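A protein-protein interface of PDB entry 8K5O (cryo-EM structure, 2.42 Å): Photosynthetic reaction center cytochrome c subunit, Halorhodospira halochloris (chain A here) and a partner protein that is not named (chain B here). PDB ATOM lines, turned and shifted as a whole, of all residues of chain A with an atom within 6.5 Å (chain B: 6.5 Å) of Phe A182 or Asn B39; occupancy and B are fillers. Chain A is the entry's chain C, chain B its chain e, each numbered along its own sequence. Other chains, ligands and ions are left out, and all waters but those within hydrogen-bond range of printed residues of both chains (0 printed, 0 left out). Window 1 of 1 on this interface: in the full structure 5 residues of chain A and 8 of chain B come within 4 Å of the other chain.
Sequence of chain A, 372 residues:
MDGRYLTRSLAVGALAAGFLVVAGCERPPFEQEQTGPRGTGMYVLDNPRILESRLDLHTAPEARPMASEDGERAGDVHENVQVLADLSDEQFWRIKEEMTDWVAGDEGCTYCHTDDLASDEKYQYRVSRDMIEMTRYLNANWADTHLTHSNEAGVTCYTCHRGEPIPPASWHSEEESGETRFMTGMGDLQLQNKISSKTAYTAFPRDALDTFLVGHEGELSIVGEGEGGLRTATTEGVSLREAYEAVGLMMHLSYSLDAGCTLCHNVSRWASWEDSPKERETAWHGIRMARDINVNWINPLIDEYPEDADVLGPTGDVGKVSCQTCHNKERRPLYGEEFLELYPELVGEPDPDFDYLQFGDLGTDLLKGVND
O of Ile B33 touches CE2 of Phe A182, 3.3 Å away.
O of Ser B34 touches CE2 of Phe A182, at 3.1 Å.
Phe A182 touches Ser B35.
Phe A182 touches Glu B36.
CG of Glu B42 touches CE1 of Phe A182, at 3.3 Å.
Met A183 touches Glu B42.
Thr A184 touches Ile B33.
Thr A184 touches Leu B41.
N of Gly A185 touches ND2 of Asn B39, 3.8 Å away.
CG of Met A186 touches CB of Ser B34, 3.7 Å away.
Phe A182 touches six residues of chain B.
Asn B39 touches three residues of chain A.
Of the printed residues of chain B, Met A186 touches Ser B34.
Of the printed residues of chain B, Gly A185 touches Ile B33 and Asn B39.
Of the printed residues of chain A, Ile B33 touches Phe A182, Thr A184 and Gly A185.
Of the printed residues of chain A, Glu B42 touches Phe A182, Met A183 and Thr A184.
Printed residues of chain A within 4 Å of Ser B35: Phe A182 (3.6 Å).
The nearest residue of chain A that does not touch Asn B39 is Met A186 (6.1 Å).
Of the 8 printed residues of chain A, 5 touch a printed residue of chain B.
Printed residues of chain A that touch a printed residue of chain B: Phe A182, Met A183, Thr A184, Gly A185 and Met A186.
Hydrophobic or aromatic side chains of chain A that line the printed part of chain B: Phe A182 and Met A186.
Hydrophobic or aromatic side chains of chain B that line the printed part of chain A: Ile B33 and Leu B41.
Among the printed residues, no Asp or Glu carboxylate lies within 4 Å of a Lys or Arg side-chain nitrogen of the other chain.
The side-chain amide oxygen of Asn B39 lies within hydrogen-bond range of the backbone NH of Glu B42, 3.3 Å away.
N of Arg B37 lies close to OG of Ser B35, 3.4 Å away.
N of Asn B39 lies within hydrogen-bond range of O of Cys B32.
The backbone NH (N) of Leu B41 is in hydrogen-bond range of the side-chain amide oxygen (OD1) of Asn B39 (3.0 Å).
The backbone carbonyl oxygen (O) of Ala B31 lies within hydrogen-bond range of the side-chain hydroxyl (OG) of Ser B34 (2.9 Å).
O of Ile B33 is in hydrogen-bond range of ND2 of Asn B39 (2.8 Å).
The backbone carbonyl oxygen of Thr A184 is in hydrogen-bond range of the side-chain amide nitrogen of Asn B39 (2.9 Å).
The side-chain hydroxyl (OG1) of Thr A184 is in hydrogen-bond range of the side-chain carboxylate (OE1) of Glu B42, 3.2 Å away.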
ATOM      1  N   THR A 180     -21.268  19.804 -21.434  1.00  0.00           N
ATOM      2  CA  THR A 180     -20.280  20.641 -22.094  1.00  0.00           C
ATOM      3  C   THR A 180     -19.014  19.834 -22.332  1.00  0.00           C
ATOM      4  O   THR A 180     -18.479  19.213 -21.411  1.00  0.00           O
ATOM      5  CB  THR A 180     -19.972  21.871 -21.247  1.00  0.00           C
ATOM      6  OG1 THR A 180     -21.143  22.691 -21.145  1.00  0.00           O
ATOM      7  CG2 THR A 180     -18.861  22.669 -21.878  1.00  0.00           C
ATOM      8  N   ARG A 181     -18.534  19.841 -23.569  1.00  0.00           N
ATOM      9  CA  ARG A 181     -17.387  19.032 -23.947  1.00  0.00           C
ATOM     10  C   ARG A 181     -16.099  19.791 -23.669  1.00  0.00           C
ATOM     11  O   ARG A 181     -15.940  20.939 -24.094  1.00  0.00           O
ATOM     12  CB  ARG A 181     -17.465  18.644 -25.422  1.00  0.00           C
ATOM     13  CG  ARG A 181     -18.407  17.494 -25.701  1.00  0.00           C
ATOM     14  CD  ARG A 181     -18.288  17.026 -27.133  1.00  0.00           C
ATOM     15  NE  ARG A 181     -17.140  16.150 -27.327  1.00  0.00           N
ATOM     16  CZ  ARG A 181     -16.713  15.729 -28.507  1.00  0.00           C
ATOM     17  NH1 ARG A 181     -17.305  16.100 -29.629  1.00  0.00           N
ATOM     18  NH2 ARG A 181     -15.667  14.910 -28.563  1.00  0.00           N
ATOM     19  N   PHE A 182     -15.192  19.149 -22.941  1.00  0.00           N
ATOM     20  CA  PHE A 182     -13.840  19.655 -22.732  1.00  0.00           C
ATOM     21  C   PHE A 182     -13.014  19.216 -23.931  1.00  0.00           C
ATOM     22  O   PHE A 182     -12.413  18.147 -23.939  1.00  0.00           O
ATOM     23  CB  PHE A 182     -13.271  19.125 -21.423  1.00  0.00           C
ATOM     24  CG  PHE A 182     -12.032  19.827 -20.969  1.00  0.00           C
ATOM     25  CD1 PHE A 182     -11.611  20.990 -21.580  1.00  0.00           C
ATOM     26  CD2 PHE A 182     -11.287  19.322 -19.925  1.00  0.00           C
ATOM     27  CE1 PHE A 182     -10.471  21.626 -21.156  1.00  0.00           C
ATOM     28  CE2 PHE A 182     -10.147  19.960 -19.502  1.00  0.00           C
ATOM     29  CZ  PHE A 182      -9.739  21.110 -20.117  1.00  0.00           C
ATOM     30  N   MET A 183     -12.974  20.065 -24.957  1.00  0.00           N
ATOM     31  CA  MET A 183     -12.458  19.630 -26.250  1.00  0.00           C
ATOM     32  C   MET A 183     -10.961  19.349 -26.217  1.00  0.00           C
ATOM     33  O   MET A 183     -10.484  18.488 -26.962  1.00  0.00           O
ATOM     34  CB  MET A 183     -12.789  20.668 -27.317  1.00  0.00           C
ATOM     35  CG  MET A 183     -14.274  20.780 -27.592  1.00  0.00           C
ATOM     36  SD  MET A 183     -15.025  19.205 -28.024  1.00  0.00           S
ATOM     37  CE  MET A 183     -14.087  18.790 -29.483  1.00  0.00           C
ATOM     38  N   THR A 184     -10.207  20.048 -25.374  1.00  0.00           N
ATOM     39  CA  THR A 184      -8.764  19.873 -25.319  1.00  0.00           C
ATOM     40  C   THR A 184      -8.341  19.076 -24.079  1.00  0.00           C
ATOM     41  O   THR A 184      -7.147  18.909 -23.825  1.00  0.00           O
ATOM     42  CB  THR A 184      -8.085  21.254 -25.377  1.00  0.00           C
ATOM     43  OG1 THR A 184      -8.465  21.907 -26.591  1.00  0.00           O
ATOM     44  CG2 THR A 184      -6.581  21.140 -25.447  1.00  0.00           C
ATOM     45  N   GLY A 185      -9.290  18.532 -23.336  1.00  0.00           N
ATOM     46  CA  GLY A 185      -8.998  17.792 -22.125  1.00  0.00           C
ATOM     47  C   GLY A 185      -8.777  16.318 -22.371  1.00  0.00           C
ATOM     48  O   GLY A 185      -8.242  15.907 -23.405  1.00  0.00           O
ATOM     49  N   MET A 186      -9.197  15.505 -21.405  1.00  0.00           N
ATOM     50  CA  MET A 186      -9.062  14.057 -21.477  1.00  0.00           C
ATOM     51  C   MET A 186     -10.406  13.399 -21.199  1.00  0.00           C
ATOM     52  O   MET A 186     -11.343  14.023 -20.696  1.00  0.00           O
ATOM     53  CB  MET A 186      -8.026  13.530 -20.478  1.00  0.00           C
ATOM     54  CG  MET A 186      -6.626  14.059 -20.660  1.00  0.00           C
ATOM     55  SD  MET A 186      -5.453  13.113 -19.687  1.00  0.00           S
ATOM     56  CE  MET A 186      -4.736  12.065 -20.942  1.00  0.00           C
ATOM     57  N   ASP A 188     -12.940  11.742 -23.161  1.00  0.00           N
ATOM     58  CA  ASP A 188     -14.165  11.892 -23.934  1.00  0.00           C
ATOM     59  C   ASP A 188     -14.339  10.627 -24.760  1.00  0.00           C
ATOM     60  O   ASP A 188     -13.579  10.381 -25.702  1.00  0.00           O
ATOM     61  CB  ASP A 188     -14.108  13.134 -24.814  1.00  0.00           C
ATOM     62  CG  ASP A 188     -15.446  13.489 -25.416  1.00  0.00           C
ATOM     63  OD1 ASP A 188     -16.425  12.744 -25.209  1.00  0.00           O
ATOM     64  OD2 ASP A 188     -15.521  14.536 -26.088  1.00  0.00           O
ATOM     65  N   ALA B  31      -2.592  15.256 -16.428  1.00  0.00           N
ATOM     66  CA  ALA B  31      -3.465  15.704 -15.349  1.00  0.00           C
ATOM     67  C   ALA B  31      -3.784  17.184 -15.486  1.00  0.00           C
ATOM     68  O   ALA B  31      -4.912  17.613 -15.225  1.00  0.00           O
ATOM     69  CB  ALA B  31      -2.823  15.416 -13.993  1.00  0.00           C
ATOM     70  N   CYS B  32      -2.792  17.982 -15.880  1.00  0.00           N
ATOM     71  CA  CYS B  32      -3.040  19.398 -16.140  1.00  0.00           C
ATOM     72  C   CYS B  32      -3.955  19.589 -17.341  1.00  0.00           C
ATOM     73  O   CYS B  32      -4.846  20.443 -17.319  1.00  0.00           O
ATOM     74  CB  CYS B  32      -1.721  20.131 -16.357  1.00  0.00           C
ATOM     75  SG  CYS B  32      -0.530  19.864 -15.064  1.00  0.00           S
ATOM     76  N   ILE B  33      -3.747  18.805 -18.400  1.00  0.00           N
ATOM     77  CA  ILE B  33      -4.566  18.918 -19.602  1.00  0.00           C
ATOM     78  C   ILE B  33      -6.018  18.589 -19.289  1.00  0.00           C
ATOM     79  O   ILE B  33      -6.942  19.271 -19.750  1.00  0.00           O
ATOM     80  CB  ILE B  33      -4.003  18.007 -20.709  1.00  0.00           C
ATOM     81  CG1 ILE B  33      -2.804  18.666 -21.391  1.00  0.00           C
ATOM     82  CG2 ILE B  33      -5.074  17.665 -21.727  1.00  0.00           C
ATOM     83  CD1 ILE B  33      -1.833  17.684 -22.013  1.00  0.00           C
ATOM     84  N   SER B  34      -6.243  17.539 -18.502  1.00  0.00           N
ATOM     85  CA  SER B  34      -7.594  17.129 -18.152  1.00  0.00           C
ATOM     86  C   SER B  34      -8.291  18.145 -17.263  1.00  0.00           C
ATOM     87  O   SER B  34      -9.519  18.110 -17.150  1.00  0.00           O
ATOM     88  CB  SER B  34      -7.559  15.769 -17.461  1.00  0.00           C
ATOM     89  OG  SER B  34      -7.006  15.880 -16.166  1.00  0.00           O
ATOM     90  N   SER B  35      -7.543  19.039 -16.630  1.00  0.00           N
ATOM     91  CA  SER B  35      -8.117  20.047 -15.755  1.00  0.00           C
ATOM     92  C   SER B  35      -8.463  21.290 -16.560  1.00  0.00           C
ATOM     93  O   SER B  35      -7.619  21.826 -17.279  1.00  0.00           O
ATOM     94  CB  SER B  35      -7.145  20.396 -14.630  1.00  0.00           C
ATOM     95  OG  SER B  35      -7.571  21.550 -13.935  1.00  0.00           O
ATOM     96  N   GLU B  36      -9.711  21.745 -16.434  1.00  0.00           N
ATOM     97  CA  GLU B  36     -10.127  22.965 -17.114  1.00  0.00           C
ATOM     98  C   GLU B  36      -9.329  24.162 -16.627  1.00  0.00           C
ATOM     99  O   GLU B  36      -8.935  25.024 -17.422  1.00  0.00           O
ATOM    100  CB  GLU B  36     -11.617  23.207 -16.892  1.00  0.00           C
ATOM    101  CG  GLU B  36     -12.131  24.441 -17.585  1.00  0.00           C
ATOM    102  CD  GLU B  36     -13.592  24.699 -17.317  1.00  0.00           C
ATOM    103  OE1 GLU B  36     -14.198  23.943 -16.530  1.00  0.00           O
ATOM    104  OE2 GLU B  36     -14.138  25.654 -17.903  1.00  0.00           O
ATOM    105  N   ARG B  37      -9.088  24.234 -15.319  1.00  0.00           N
ATOM    106  CA  ARG B  37      -8.342  25.352 -14.761  1.00  0.00           C
ATOM    107  C   ARG B  37      -6.916  25.380 -15.286  1.00  0.00           C
ATOM    108  O   ARG B  37      -6.366  26.452 -15.554  1.00  0.00           O
ATOM    109  CB  ARG B  37      -8.349  25.263 -13.238  1.00  0.00           C
ATOM    110  CG  ARG B  37      -7.411  26.218 -12.554  1.00  0.00           C
ATOM    111  CD  ARG B  37      -7.562  26.091 -11.066  1.00  0.00           C
ATOM    112  NE  ARG B  37      -6.648  26.950 -10.329  1.00  0.00           N
ATOM    113  CZ  ARG B  37      -6.841  28.245 -10.130  1.00  0.00           C
ATOM    114  NH1 ARG B  37      -7.881  28.876 -10.647  1.00  0.00           N
ATOM    115  NH2 ARG B  37      -5.973  28.921  -9.388  1.00  0.00           N
ATOM    116  N   PHE B  38      -6.311  24.214 -15.455  1.00  0.00           N
ATOM    117  CA  PHE B  38      -4.886  24.109 -15.708  1.00  0.00           C
ATOM    118  C   PHE B  38      -4.544  23.721 -17.138  1.00  0.00           C
ATOM    119  O   PHE B  38      -3.361  23.627 -17.469  1.00  0.00           O
ATOM    120  CB  PHE B  38      -4.282  23.099 -14.741  1.00  0.00           C
ATOM    121  CG  PHE B  38      -4.505  23.442 -13.299  1.00  0.00           C
ATOM    122  CD1 PHE B  38      -4.150  24.685 -12.808  1.00  0.00           C
ATOM    123  CD2 PHE B  38      -5.047  22.512 -12.428  1.00  0.00           C
ATOM    124  CE1 PHE B  38      -4.329  24.990 -11.481  1.00  0.00           C
ATOM    125  CE2 PHE B  38      -5.235  22.818 -11.100  1.00  0.00           C
ATOM    126  CZ  PHE B  38      -4.877  24.058 -10.628  1.00  0.00           C
ATOM    127  N   ASN B  39      -5.487  23.430 -17.985  1.00  0.00           N
ATOM    128  CA  ASN B  39      -5.192  23.171 -19.356  1.00  0.00           C
ATOM    129  C   ASN B  39      -4.848  24.473 -20.046  1.00  0.00           C
ATOM    130  O   ASN B  39      -5.696  25.278 -20.272  1.00  0.00           O
ATOM    131  CB  ASN B  39      -6.333  22.401 -20.029  1.00  0.00           C
ATOM    132  CG  ASN B  39      -5.950  21.819 -21.350  1.00  0.00           C
ATOM    133  OD1 ASN B  39      -4.866  22.044 -21.849  1.00  0.00           O
ATOM    134  ND2 ASN B  39      -6.852  21.075 -21.931  1.00  0.00           N
ATOM    135  N   TRP B  40      -3.592  24.690 -20.302  1.00  0.00           N
ATOM    136  CA  TRP B  40      -3.102  25.840 -21.047  1.00  0.00           C
ATOM    137  C   TRP B  40      -3.413  25.716 -22.530  1.00  0.00           C
ATOM    138  O   TRP B  40      -3.516  26.728 -23.231  1.00  0.00           O
ATOM    139  CB  TRP B  40      -1.599  25.992 -20.825  1.00  0.00           C
ATOM    140  CG  TRP B  40      -0.799  24.893 -21.459  1.00  0.00           C
ATOM    141  CD1 TRP B  40      -0.016  24.991 -22.566  1.00  0.00           C
ATOM    142  CD2 TRP B  40      -0.711  23.529 -21.025  1.00  0.00           C
ATOM    143  NE1 TRP B  40       0.555  23.778 -22.850  1.00  0.00           N
ATOM    144  CE2 TRP B  40       0.145  22.863 -21.918  1.00  0.00           C
ATOM    145  CE3 TRP B  40      -1.268  22.808 -19.962  1.00  0.00           C
ATOM    146  CZ2 TRP B  40       0.453  21.513 -21.787  1.00  0.00           C
ATOM    147  CZ3 TRP B  40      -0.960  21.472 -19.835  1.00  0.00           C
ATOM    148  CH2 TRP B  40      -0.105  20.837 -20.739  1.00  0.00           C
ATOM    149  N   LEU B  41      -3.546  24.486 -23.024  1.00  0.00           N
ATOM    150  CA  LEU B  41      -3.883  24.277 -24.425  1.00  0.00           C
ATOM    151  C   LEU B  41      -5.333  24.648 -24.703  1.00  0.00           C
ATOM    152  O   LEU B  41      -5.644  25.212 -25.758  1.00  0.00           O
ATOM    153  CB  LEU B  41      -3.604  22.826 -24.808  1.00  0.00           C
ATOM    154  CG  LEU B  41      -2.159  22.365 -24.617  1.00  0.00           C
ATOM    155  CD1 LEU B  41      -2.058  20.864 -24.730  1.00  0.00           C
ATOM    156  CD2 LEU B  41      -1.234  23.037 -25.613  1.00  0.00           C
ATOM    157  N   GLU B  42      -6.236  24.322 -23.778  1.00  0.00           N
ATOM    158  CA  GLU B  42      -7.608  24.811 -23.843  1.00  0.00           C
ATOM    159  C   GLU B  42      -7.666  26.311 -23.586  1.00  0.00           C
ATOM    160  O   GLU B  42      -8.404  27.033 -24.263  1.00  0.00           O
ATOM    161  CB  GLU B  42      -8.467  24.064 -22.825  1.00  0.00           C
ATOM    162  CG  GLU B  42      -9.900  24.555 -22.666  1.00  0.00           C
ATOM    163  CD  GLU B  42     -10.815  24.126 -23.794  1.00  0.00           C
ATOM    164  OE1 GLU B  42     -10.508  23.124 -24.470  1.00  0.00           O
ATOM    165  OE2 GLU B  42     -11.869  24.767 -23.976  1.00  0.00           O
ATOM    166  N   GLY B  43      -6.885  26.789 -22.624  1.00  0.00           N
ATOM    167  CA  GLY B  43      -6.863  28.195 -22.263  1.00  0.00           C
ATOM    168  C   GLY B  43      -8.116  28.709 -21.591  1.00  0.00           C
ATOM    169  O   GLY B  43      -8.526  29.847 -21.845  1.00  0.00           O
ATOM    170  N   ALA B  44      -8.725  27.908 -20.725  1.00  0.00           N
ATOM    171  CA  ALA B  44      -9.921  28.340 -20.026  1.00  0.00           C
ATOM    172  C   ALA B  44      -9.583  29.420 -19.000  1.00  0.00           C
ATOM    173  O   ALA B  44      -8.460  29.479 -18.495  1.00  0.00           O
ATOM    174  CB  ALA B  44     -10.589  27.157 -19.336  1.00  0.00           C
